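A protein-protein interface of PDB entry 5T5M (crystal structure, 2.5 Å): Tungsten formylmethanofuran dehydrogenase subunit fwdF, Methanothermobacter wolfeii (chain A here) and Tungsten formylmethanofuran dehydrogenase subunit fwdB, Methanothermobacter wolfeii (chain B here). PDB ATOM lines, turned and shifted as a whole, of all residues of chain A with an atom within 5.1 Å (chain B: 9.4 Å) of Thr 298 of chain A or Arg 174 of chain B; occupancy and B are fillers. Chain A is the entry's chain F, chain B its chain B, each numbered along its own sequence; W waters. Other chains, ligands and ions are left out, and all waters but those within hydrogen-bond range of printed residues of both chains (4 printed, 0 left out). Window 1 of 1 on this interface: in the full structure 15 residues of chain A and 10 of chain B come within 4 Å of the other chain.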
ATOM      1  N   ALA A 273      21.916  -6.183   5.988  1.00  0.00           N
ATOM      2  CA  ALA A 273      21.290  -5.018   6.615  1.00  0.00           C
ATOM      3  C   ALA A 273      22.300  -3.901   6.856  1.00  0.00           C
ATOM      4  O   ALA A 273      22.397  -3.351   7.953  1.00  0.00           O
ATOM      5  CB  ALA A 273      20.592  -5.406   7.920  1.00  0.00           C
ATOM      6  N   PHE A 288      13.519  -0.711   7.331  1.00  0.00           N
ATOM      7  CA  PHE A 288      13.853  -1.667   8.385  1.00  0.00           C
ATOM      8  C   PHE A 288      12.744  -1.658   9.433  1.00  0.00           C
ATOM      9  O   PHE A 288      12.806  -0.883  10.398  1.00  0.00           O
ATOM     10  CB  PHE A 288      15.194  -1.312   9.036  1.00  0.00           C
ATOM     11  CG  PHE A 288      16.415  -1.625   8.201  1.00  0.00           C
ATOM     12  CD1 PHE A 288      16.369  -2.545   7.163  1.00  0.00           C
ATOM     13  CD2 PHE A 288      17.638  -1.020   8.494  1.00  0.00           C
ATOM     14  CE1 PHE A 288      17.508  -2.830   6.420  1.00  0.00           C
ATOM     15  CE2 PHE A 288      18.787  -1.321   7.747  1.00  0.00           C
ATOM     16  CZ  PHE A 288      18.714  -2.214   6.718  1.00  0.00           C
ATOM     17  N   PRO A 289      11.725  -2.508   9.314  1.00  0.00           N
ATOM     18  CA  PRO A 289      10.644  -2.499  10.310  1.00  0.00           C
ATOM     19  C   PRO A 289      11.173  -2.779  11.710  1.00  0.00           C
ATOM     20  O   PRO A 289      12.111  -3.557  11.900  1.00  0.00           O
ATOM     21  CB  PRO A 289       9.700  -3.610   9.832  1.00  0.00           C
ATOM     22  CG  PRO A 289      10.074  -3.891   8.412  1.00  0.00           C
ATOM     23  CD  PRO A 289      11.539  -3.554   8.294  1.00  0.00           C
ATOM     24  N   LYS A 290      10.573  -2.135  12.686  1.00  0.00           N
ATOM     25  CA  LYS A 290      10.898  -2.361  14.088  1.00  0.00           C
ATOM     26  C   LYS A 290       9.937  -3.394  14.675  1.00  0.00           C
ATOM     27  O   LYS A 290       8.740  -3.361  14.377  1.00  0.00           O
ATOM     28  CB  LYS A 290      10.803  -1.061  14.872  1.00  0.00           C
ATOM     29  CG  LYS A 290      11.544  -1.056  16.211  1.00  0.00           C
ATOM     30  CD  LYS A 290      12.872  -0.274  16.136  1.00  0.00           C
ATOM     31  CE  LYS A 290      13.809  -0.542  17.338  1.00  0.00           C
ATOM     32  NZ  LYS A 290      14.351  -1.945  17.406  1.00  0.00           N
ATOM     33  N   PRO A 291      10.400  -4.348  15.483  1.00  0.00           N
ATOM     34  CA  PRO A 291       9.468  -5.319  16.069  1.00  0.00           C
ATOM     35  C   PRO A 291       8.498  -4.646  17.026  1.00  0.00           C
ATOM     36  O   PRO A 291       8.864  -3.735  17.770  1.00  0.00           O
ATOM     37  CB  PRO A 291      10.392  -6.314  16.794  1.00  0.00           C
ATOM     38  CG  PRO A 291      11.683  -5.617  16.951  1.00  0.00           C
ATOM     39  CD  PRO A 291      11.799  -4.693  15.776  1.00  0.00           C
ATOM     40  N   GLU A 296       9.825 -10.616  19.166  1.00  0.00           N
ATOM     41  CA  GLU A 296       9.194 -10.724  17.865  1.00  0.00           C
ATOM     42  C   GLU A 296      10.235 -10.400  16.806  1.00  0.00           C
ATOM     43  O   GLU A 296      11.063  -9.501  16.992  1.00  0.00           O
ATOM     44  CB  GLU A 296       8.005  -9.762  17.788  1.00  0.00           C
ATOM     45  CG  GLU A 296       7.022  -9.999  16.663  1.00  0.00           C
ATOM     46  CD  GLU A 296       6.885  -8.792  15.732  1.00  0.00           C
ATOM     47  OE1 GLU A 296       7.134  -8.936  14.509  1.00  0.00           O
ATOM     48  OE2 GLU A 296       6.531  -7.695  16.226  1.00  0.00           O
ATOM     49  N   LYS A 297      10.223 -11.154  15.715  1.00  0.00           N
ATOM     50  CA  LYS A 297      11.143 -10.909  14.619  1.00  0.00           C
ATOM     51  C   LYS A 297      10.397 -10.315  13.433  1.00  0.00           C
ATOM     52  O   LYS A 297       9.197 -10.541  13.248  1.00  0.00           O
ATOM     53  CB  LYS A 297      11.865 -12.186  14.199  1.00  0.00           C
ATOM     54  CG  LYS A 297      12.892 -12.686  15.212  1.00  0.00           C
ATOM     55  CD  LYS A 297      14.155 -13.144  14.504  1.00  0.00           C
ATOM     56  CE  LYS A 297      14.961 -14.112  15.345  1.00  0.00           C
ATOM     57  NZ  LYS A 297      16.103 -14.665  14.566  1.00  0.00           N
ATOM     58  N   THR A 298      11.124  -9.528  12.649  1.00  0.00           N
ATOM     59  CA  THR A 298      10.578  -8.814  11.507  1.00  0.00           C
ATOM     60  C   THR A 298      11.309  -9.222  10.238  1.00  0.00           C
ATOM     61  O   THR A 298      12.393  -9.809  10.271  1.00  0.00           O
ATOM     62  CB  THR A 298      10.708  -7.296  11.671  1.00  0.00           C
ATOM     63  OG1 THR A 298      12.094  -6.954  11.810  1.00  0.00           O
ATOM     64  CG2 THR A 298       9.957  -6.795  12.883  1.00  0.00           C
ATOM     65  N   THR A 299      10.697  -8.892   9.110  1.00  0.00           N
ATOM     66  CA  THR A 299      11.392  -8.981   7.840  1.00  0.00           C
ATOM     67  C   THR A 299      12.602  -8.055   7.845  1.00  0.00           C
ATOM     68  O   THR A 299      12.482  -6.865   8.136  1.00  0.00           O
ATOM     69  CB  THR A 299      10.441  -8.608   6.714  1.00  0.00           C
ATOM     70  OG1 THR A 299       9.234  -9.356   6.869  1.00  0.00           O
ATOM     71  CG2 THR A 299      11.062  -8.899   5.364  1.00  0.00           C
ATOM     72  N   LYS A 300      13.767  -8.605   7.503  1.00  0.00           N
ATOM     73  CA  LYS A 300      15.010  -7.842   7.565  1.00  0.00           C
ATOM     74  C   LYS A 300      14.970  -6.622   6.646  1.00  0.00           C
ATOM     75  O   LYS A 300      15.333  -5.514   7.054  1.00  0.00           O
ATOM     76  CB  LYS A 300      16.185  -8.748   7.206  1.00  0.00           C
ATOM     77  CG  LYS A 300      17.539  -8.186   7.594  1.00  0.00           C
ATOM     78  CD  LYS A 300      18.673  -9.056   7.070  1.00  0.00           C
ATOM     79  CE  LYS A 300      18.725 -10.396   7.756  1.00  0.00           C
ATOM     80  NZ  LYS A 300      19.621 -11.318   7.023  1.00  0.00           N
ATOM     81  N   LEU A 301      14.571  -6.813   5.389  1.00  0.00           N
ATOM     82  CA  LEU A 301      14.468  -5.728   4.414  1.00  0.00           C
ATOM     83  C   LEU A 301      13.049  -5.722   3.865  1.00  0.00           C
ATOM     84  O   LEU A 301      12.658  -6.634   3.127  1.00  0.00           O
ATOM     85  CB  LEU A 301      15.492  -5.885   3.288  1.00  0.00           C
ATOM     86  CG  LEU A 301      15.544  -4.754   2.250  1.00  0.00           C
ATOM     87  CD1 LEU A 301      15.921  -3.408   2.880  1.00  0.00           C
ATOM     88  CD2 LEU A 301      16.504  -5.087   1.114  1.00  0.00           C
ATOM     89  N   LYS B 140      24.392  -8.013  22.832  1.00  0.00           N
ATOM     90  CA  LYS B 140      24.538  -8.305  21.410  1.00  0.00           C
ATOM     91  C   LYS B 140      23.240  -8.821  20.795  1.00  0.00           C
ATOM     92  O   LYS B 140      22.867  -8.410  19.692  1.00  0.00           O
ATOM     93  CB  LYS B 140      25.657  -9.324  21.201  1.00  0.00           C
ATOM     94  CG  LYS B 140      25.805  -9.762  19.758  1.00  0.00           C
ATOM     95  CD  LYS B 140      27.151 -10.413  19.486  1.00  0.00           C
ATOM     96  CE  LYS B 140      27.118 -11.903  19.676  1.00  0.00           C
ATOM     97  NZ  LYS B 140      28.165 -12.537  18.836  1.00  0.00           N
ATOM     98  N   ASN B 141      22.544  -9.728  21.484  1.00  0.00           N
ATOM     99  CA  ASN B 141      21.392 -10.390  20.885  1.00  0.00           C
ATOM    100  C   ASN B 141      20.056  -9.705  21.156  1.00  0.00           C
ATOM    101  O   ASN B 141      19.107  -9.948  20.403  1.00  0.00           O
ATOM    102  CB  ASN B 141      21.324 -11.847  21.361  1.00  0.00           C
ATOM    103  CG  ASN B 141      22.471 -12.678  20.835  1.00  0.00           C
ATOM    104  OD1 ASN B 141      22.590 -12.886  19.630  1.00  0.00           O
ATOM    105  ND2 ASN B 141      23.324 -13.158  21.734  1.00  0.00           N
ATOM    106  N   ALA B 143      19.714  -6.010  22.722  1.00  0.00           N
ATOM    107  CA  ALA B 143      19.658  -4.577  23.014  1.00  0.00           C
ATOM    108  C   ALA B 143      19.263  -3.748  21.788  1.00  0.00           C
ATOM    109  O   ALA B 143      19.843  -3.893  20.705  1.00  0.00           O
ATOM    110  CB  ALA B 143      21.013  -4.091  23.544  1.00  0.00           C
ATOM    111  N   ASP B 144      18.295  -2.843  21.980  1.00  0.00           N
ATOM    112  CA  ASP B 144      17.934  -1.867  20.968  1.00  0.00           C
ATOM    113  C   ASP B 144      18.143  -0.424  21.419  1.00  0.00           C
ATOM    114  O   ASP B 144      17.971   0.495  20.606  1.00  0.00           O
ATOM    115  CB  ASP B 144      16.482  -2.068  20.514  1.00  0.00           C
ATOM    116  CG  ASP B 144      15.465  -1.919  21.631  1.00  0.00           C
ATOM    117  OD1 ASP B 144      15.831  -1.889  22.834  1.00  0.00           O
ATOM    118  OD2 ASP B 144      14.269  -1.863  21.289  1.00  0.00           O
ATOM    119  N   VAL B 165      27.635  -3.286  19.439  1.00  0.00           N
ATOM    120  CA  VAL B 165      26.690  -2.407  18.749  1.00  0.00           C
ATOM    121  C   VAL B 165      26.603  -2.738  17.258  1.00  0.00           C
ATOM    122  O   VAL B 165      25.517  -2.982  16.730  1.00  0.00           O
ATOM    123  CB  VAL B 165      27.055  -0.924  18.965  1.00  0.00           C
ATOM    124  CG1 VAL B 165      26.031  -0.027  18.289  1.00  0.00           C
ATOM    125  CG2 VAL B 165      27.156  -0.626  20.448  1.00  0.00           C
ATOM    126  N   PHE B 166      27.737  -2.712  16.553  1.00  0.00           N
ATOM    127  CA  PHE B 166      27.712  -3.041  15.135  1.00  0.00           C
ATOM    128  C   PHE B 166      27.457  -4.521  14.920  1.00  0.00           C
ATOM    129  O   PHE B 166      26.906  -4.908  13.885  1.00  0.00           O
ATOM    130  CB  PHE B 166      29.022  -2.616  14.479  1.00  0.00           C
ATOM    131  CG  PHE B 166      29.197  -1.127  14.411  1.00  0.00           C
ATOM    132  CD1 PHE B 166      28.706  -0.410  13.329  1.00  0.00           C
ATOM    133  CD2 PHE B 166      29.831  -0.439  15.435  1.00  0.00           C
ATOM    134  CE1 PHE B 166      28.852   0.959  13.266  1.00  0.00           C
ATOM    135  CE2 PHE B 166      29.984   0.926  15.375  1.00  0.00           C
ATOM    136  CZ  PHE B 166      29.495   1.629  14.290  1.00  0.00           C
ATOM    137  N   ALA B 167      27.825  -5.344  15.899  1.00  0.00           N
ATOM    138  CA  ALA B 167      27.551  -6.774  15.857  1.00  0.00           C
ATOM    139  C   ALA B 167      26.076  -7.051  15.602  1.00  0.00           C
ATOM    140  O   ALA B 167      25.194  -6.366  16.129  1.00  0.00           O
ATOM    141  CB  ALA B 167      27.962  -7.414  17.183  1.00  0.00           C
ATOM    142  N   ARG B 168      25.815  -8.082  14.806  1.00  0.00           N
ATOM    143  CA  ARG B 168      24.456  -8.545  14.570  1.00  0.00           C
ATOM    144  C   ARG B 168      24.161  -9.680  15.535  1.00  0.00           C
ATOM    145  O   ARG B 168      25.006 -10.551  15.754  1.00  0.00           O
ATOM    146  CB  ARG B 168      24.274  -8.998  13.126  1.00  0.00           C
ATOM    147  CG  ARG B 168      24.669  -7.949  12.102  1.00  0.00           C
ATOM    148  CD  ARG B 168      24.972  -8.599  10.769  1.00  0.00           C
ATOM    149  NE  ARG B 168      25.438  -7.630   9.782  1.00  0.00           N
ATOM    150  CZ  ARG B 168      26.664  -7.128   9.766  1.00  0.00           C
ATOM    151  NH1 ARG B 168      27.549  -7.489  10.685  1.00  0.00           N
ATOM    152  NH2 ARG B 168      26.998  -6.248   8.842  1.00  0.00           N
ATOM    153  N   GLY B 169      22.982  -9.640  16.148  1.00  0.00           N
ATOM    154  CA  GLY B 169      22.588 -10.619  17.131  1.00  0.00           C
ATOM    155  C   GLY B 169      21.256 -11.245  16.772  1.00  0.00           C
ATOM    156  O   GLY B 169      20.602 -10.868  15.794  1.00  0.00           O
ATOM    157  N   PHE B 170      20.856 -12.205  17.604  1.00  0.00           N
ATOM    158  CA  PHE B 170      19.734 -13.062  17.236  1.00  0.00           C
ATOM    159  C   PHE B 170      18.457 -12.256  17.026  1.00  0.00           C
ATOM    160  O   PHE B 170      17.785 -12.405  16.003  1.00  0.00           O
ATOM    161  CB  PHE B 170      19.518 -14.145  18.290  1.00  0.00           C
ATOM    162  CG  PHE B 170      18.504 -15.161  17.878  1.00  0.00           C
ATOM    163  CD1 PHE B 170      18.780 -16.043  16.842  1.00  0.00           C
ATOM    164  CD2 PHE B 170      17.268 -15.216  18.495  1.00  0.00           C
ATOM    165  CE1 PHE B 170      17.840 -16.980  16.435  1.00  0.00           C
ATOM    166  CE2 PHE B 170      16.327 -16.145  18.100  1.00  0.00           C
ATOM    167  CZ  PHE B 170      16.615 -17.036  17.059  1.00  0.00           C
ATOM    168  N   PHE B 171      18.092 -11.406  17.991  1.00  0.00           N
ATOM    169  CA  PHE B 171      16.933 -10.531  17.855  1.00  0.00           C
ATOM    170  C   PHE B 171      17.303  -9.150  17.327  1.00  0.00           C
ATOM    171  O   PHE B 171      16.434  -8.273  17.261  1.00  0.00           O
ATOM    172  CB  PHE B 171      16.200 -10.382  19.197  1.00  0.00           C
ATOM    173  CG  PHE B 171      15.763 -11.685  19.799  1.00  0.00           C
ATOM    174  CD1 PHE B 171      14.598 -12.302  19.385  1.00  0.00           C
ATOM    175  CD2 PHE B 171      16.520 -12.294  20.777  1.00  0.00           C
ATOM    176  CE1 PHE B 171      14.207 -13.503  19.934  1.00  0.00           C
ATOM    177  CE2 PHE B 171      16.131 -13.487  21.325  1.00  0.00           C
ATOM    178  CZ  PHE B 171      14.973 -14.095  20.903  1.00  0.00           C
ATOM    179  N   ARG B 172      18.573  -8.937  16.970  1.00  0.00           N
ATOM    180  CA  ARG B 172      19.062  -7.670  16.428  1.00  0.00           C
ATOM    181  C   ARG B 172      19.937  -7.963  15.213  1.00  0.00           C
ATOM    182  O   ARG B 172      21.131  -7.657  15.167  1.00  0.00           O
ATOM    183  CB  ARG B 172      19.845  -6.865  17.472  1.00  0.00           C
ATOM    184  CG  ARG B 172      19.068  -6.514  18.734  1.00  0.00           C
ATOM    185  CD  ARG B 172      17.867  -5.621  18.445  1.00  0.00           C
ATOM    186  NE  ARG B 172      16.973  -5.607  19.599  1.00  0.00           N
ATOM    187  CZ  ARG B 172      15.644  -5.596  19.542  1.00  0.00           C
ATOM    188  NH1 ARG B 172      15.009  -5.592  18.375  1.00  0.00           N
ATOM    189  NH2 ARG B 172      14.949  -5.600  20.671  1.00  0.00           N
ATOM    190  N   GLU B 173      19.316  -8.563  14.201  1.00  0.00           N
ATOM    191  CA  GLU B 173      20.082  -9.029  13.057  1.00  0.00           C
ATOM    192  C   GLU B 173      20.552  -7.897  12.152  1.00  0.00           C
ATOM    193  O   GLU B 173      21.389  -8.144  11.280  1.00  0.00           O
ATOM    194  CB  GLU B 173      19.280 -10.064  12.257  1.00  0.00           C
ATOM    195  CG  GLU B 173      17.831  -9.754  11.931  1.00  0.00           C
ATOM    196  CD  GLU B 173      17.141 -10.894  11.127  1.00  0.00           C
ATOM    197  OE1 GLU B 173      17.755 -11.969  10.916  1.00  0.00           O
ATOM    198  OE2 GLU B 173      15.977 -10.713  10.703  1.00  0.00           O
ATOM    199  N   ARG B 174      20.085  -6.665  12.345  1.00  0.00           N
ATOM    200  CA  ARG B 174      20.574  -5.549  11.545  1.00  0.00           C
ATOM    201  C   ARG B 174      21.721  -4.793  12.211  1.00  0.00           C
ATOM    202  O   ARG B 174      22.146  -3.751  11.700  1.00  0.00           O
ATOM    203  CB  ARG B 174      19.432  -4.578  11.220  1.00  0.00           C
ATOM    204  CG  ARG B 174      18.169  -5.253  10.705  1.00  0.00           C
ATOM    205  CD  ARG B 174      17.275  -4.266  10.000  1.00  0.00           C
ATOM    206  NE  ARG B 174      15.954  -4.808   9.685  1.00  0.00           N
ATOM    207  CZ  ARG B 174      14.917  -4.823  10.521  1.00  0.00           C
ATOM    208  NH1 ARG B 174      15.019  -4.347  11.752  1.00  0.00           N
ATOM    209  NH2 ARG B 174      13.767  -5.327  10.123  1.00  0.00           N
ATOM    210  N   GLY B 175      22.237  -5.290  13.324  1.00  0.00           N
ATOM    211  CA  GLY B 175      23.429  -4.692  13.905  1.00  0.00           C
ATOM    212  C   GLY B 175      23.204  -3.257  14.331  1.00  0.00           C
ATOM    213  O   GLY B 175      22.312  -2.942  15.132  1.00  0.00           O
ATOM    214  N   ARG B 176      24.038  -2.365  13.798  1.00  0.00           N
ATOM    215  CA  ARG B 176      23.987  -0.961  14.192  1.00  0.00           C
ATOM    216  C   ARG B 176      22.616  -0.363  13.910  1.00  0.00           C
ATOM    217  O   ARG B 176      22.083   0.401  14.726  1.00  0.00           O
ATOM    218  CB  ARG B 176      25.092  -0.193  13.462  1.00  0.00           C
ATOM    219  CG  ARG B 176      25.110   1.284  13.669  1.00  0.00           C
ATOM    220  CD  ARG B 176      25.438   1.676  15.102  1.00  0.00           C
ATOM    221  NE  ARG B 176      25.356   3.127  15.289  1.00  0.00           N
ATOM    222  CZ  ARG B 176      24.255   3.789  15.648  1.00  0.00           C
ATOM    223  NH1 ARG B 176      23.117   3.147  15.862  1.00  0.00           N
ATOM    224  NH2 ARG B 176      24.291   5.103  15.794  1.00  0.00           N
ATOM    225  N   SER B 177      22.016  -0.735  12.777  1.00  0.00           N
ATOM    226  CA  SER B 177      20.736  -0.181  12.358  1.00  0.00           C
ATOM    227  C   SER B 177      19.569  -0.594  13.252  1.00  0.00           C
ATOM    228  O   SER B 177      18.485  -0.016  13.117  1.00  0.00           O
ATOM    229  CB  SER B 177      20.429  -0.600  10.921  1.00  0.00           C
ATOM    230  OG  SER B 177      21.443  -0.180  10.011  1.00  0.00           O
ATOM    231  N   ASP B 178      19.742  -1.576  14.139  1.00  0.00           N
ATOM    232  CA  ASP B 178      18.686  -1.983  15.065  1.00  0.00           C
ATOM    233  C   ASP B 178      18.813  -1.335  16.441  1.00  0.00           C
ATOM    234  O   ASP B 178      18.010  -1.636  17.326  1.00  0.00           O
ATOM    235  CB  ASP B 178      18.669  -3.516  15.233  1.00  0.00           C
ATOM    236  CG  ASP B 178      17.858  -4.229  14.153  1.00  0.00           C
ATOM    237  OD1 ASP B 178      17.063  -3.569  13.457  1.00  0.00           O
ATOM    238  OD2 ASP B 178      18.013  -5.463  13.994  1.00  0.00           O
ATOM    239  N   ARG B 179      19.787  -0.460  16.650  1.00  0.00           N
ATOM    240  CA  ARG B 179      20.058   0.081  17.975  1.00  0.00           C
ATOM    241  C   ARG B 179      20.081   1.606  17.977  1.00  0.00           C
ATOM    242  O   ARG B 179      20.679   2.238  17.100  1.00  0.00           O
ATOM    243  CB  ARG B 179      21.392  -0.436  18.493  1.00  0.00           C
ATOM    244  CG  ARG B 179      21.600  -1.930  18.249  1.00  0.00           C
ATOM    245  CD  ARG B 179      22.861  -2.417  18.927  1.00  0.00           C
ATOM    246  NE  ARG B 179      23.295  -3.715  18.418  1.00  0.00           N
ATOM    247  CZ  ARG B 179      23.052  -4.881  19.008  1.00  0.00           C
ATOM    248  NH1 ARG B 179      22.364  -4.941  20.145  1.00  0.00           N
ATOM    249  NH2 ARG B 179      23.513  -5.993  18.459  1.00  0.00           N
ATOM    250  N   GLN B 246      13.022  -2.126  24.094  1.00  0.00           N
ATOM    251  CA  GLN B 246      12.723  -3.521  24.395  1.00  0.00           C
ATOM    252  C   GLN B 246      13.784  -4.132  25.285  1.00  0.00           C
ATOM    253  O   GLN B 246      13.490  -5.052  26.054  1.00  0.00           O
ATOM    254  CB  GLN B 246      12.600  -4.338  23.111  1.00  0.00           C
ATOM    255  CG  GLN B 246      11.539  -3.814  22.184  1.00  0.00           C
ATOM    256  CD  GLN B 246      11.247  -4.749  21.016  1.00  0.00           C
ATOM    257  OE1 GLN B 246      12.034  -5.638  20.701  1.00  0.00           O
ATOM    258  NE2 GLN B 246      10.107  -4.542  20.370  1.00  0.00           N
HETATM  259  O   HOH W   1      13.674 -12.044  10.474  1.00  0.00           O
HETATM  260  O   HOH W   2      15.101  -8.234  11.211  1.00  0.00           O
HETATM  261  O   HOH W   3      24.449  -4.428   9.830  1.00  0.00           O
HETATM  262  O   HOH W   4      12.467  -8.114  19.816  1.00  0.00           O
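The side-chain carboxylate (OD2) of Asp 144 of chain B is in salt-bridge range of the side-chain amino group (NZ) of Lys 290 of chain A (3.9 Å). O of Phe 170 of chain B is in hydrogen-bond range of NZ of Lys 297 of chain A (3.2 Å). NH2 of Arg 174 of chain B lies within hydrogen-bond range of O of Pro 289 of chain A, 3.0 Å away. The side-chain hydroxyl of Thr 298 of chain A is in hydrogen-bond range of the guanidinium group of Arg 174 of chain B. NH2 of Arg 174 of chain B sits at hydrogen-bond distance from O of Thr 299 of chain A. The backbone carbonyl oxygen (O) of Lys 300 of chain A sits at hydrogen-bond distance from the guanidinium group (NE) of Arg 174 of chain B (2.8 Å). The side-chain amide nitrogen (NE2) of Gln 246 of chain B is in hydrogen-bond range of the backbone carbonyl oxygen (O) of Pro 291 of chain A (3.0 Å).
OD1 of Asn 141 of chain B sits at hydrogen-bond distance from N of Phe 170 of chain B (2.8 Å). The guanidinium group of Arg 172 of chain B lies within salt-bridge range of the side-chain carboxylate of Asp 144 of chain B, 3.8 Å away. The backbone NH (N) of Gln 246 of chain B is in hydrogen-bond range of the side-chain carboxylate (OD2) of Asp 144 of chain B (3.1 Å). The side-chain carboxylate of Asp 178 of chain B sits at hydrogen-bond distance from the backbone NH of Glu 173 of chain B. NH1 of Arg 174 of chain B is in salt-bridge range of OD1 of Asp 178 of chain B, at 2.8 Å. OG1 of Thr 298 of chain A sits at hydrogen-bond distance from O of Pro 289 of chain A (3.4 Å).
Among the printed residues, merely in contact across the chains: Ala 273 of chain A with Arg 174 of chain B, Ala 273 of chain A with Ser 177 of chain B, Phe 288 of chain A with Arg 174 of chain B, Phe 288 of chain A with Ser 177 of chain B, Lys 290 of chain A with Arg 172 of chain B, Lys 290 of chain A with Asp 178 of chain B, Pro 291 of chain A with Arg 172 of chain B, Thr 298 of chain A with Glu 173 of chain B and Lys 300 of chain A with Glu 173 of chain B.
Thr 298 of chain A touches just these residues of chain B: Glu 173 and Arg 174. Arg 174 of chain B touches just these residues of chain A: Ala 273, Phe 288, Pro 289, Thr 298, Thr 299 and Lys 300. Of chain B, only Arg 174 (2.8 Å) comes within 4 Å of Thr 299 of chain A. Printed residues of chain A within 4 Å of Asp 178 of chain B: Lys 290 (3.7 Å). Printed residues of chain A within 4 Å of Glu 173 of chain B: Thr 298 (3.7 Å) and Lys 300 (3.7 Å). Of the printed residues of chain B, Lys 300 of chain A touches Glu 173 and Arg 174. Arg 179 of chain B touches none of the printed residues of chain A. Arg 176 of chain B touches none of the printed residues of chain A. The nearest residue of chain B that does not touch Thr 298 of chain A is Asp 178 of chain B (6.2 Å). The nearest printed residue of chain B that does not touch Lys 297 of chain A is Phe 171 of chain B (4.4 Å).
Printed residues of chain B that touch a printed residue of chain A: Asp 144, Phe 170, Arg 172, Glu 173, Arg 174, Ser 177, Asp 178 and Gln 246. Of the 11 printed residues of chain A, 9 touch a printed residue of chain B. Printed residues of chain A that touch a printed residue of chain B: Ala 273, Phe 288, Pro 289, Lys 290, Pro 291, Lys 297, Thr 298, Thr 299 and Lys 300.
Water W1 bridges O of Thr 298 of chain A (2.6 Å) and OE2 of Glu 173 of chain B (2.7 Å). Water W4 bridges OE1 of Gln 246 of chain B (2.7 Å) and O of Glu 296 of chain A (3.4 Å). Water W2 lies within hydrogen-bond range of OE2 of Glu 173 of chain B (2.7 Å), O of Thr 298 of chain A (3.3 Å) and NH2 of Arg 174 of chain B (3.4 Å). Water W3 lies within hydrogen-bond range of O of Ala 273 of chain A (3.0 Å), O of Arg 174 of chain B (3.0 Å) and NH2 of Arg 168 of chain B (3.3 Å).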
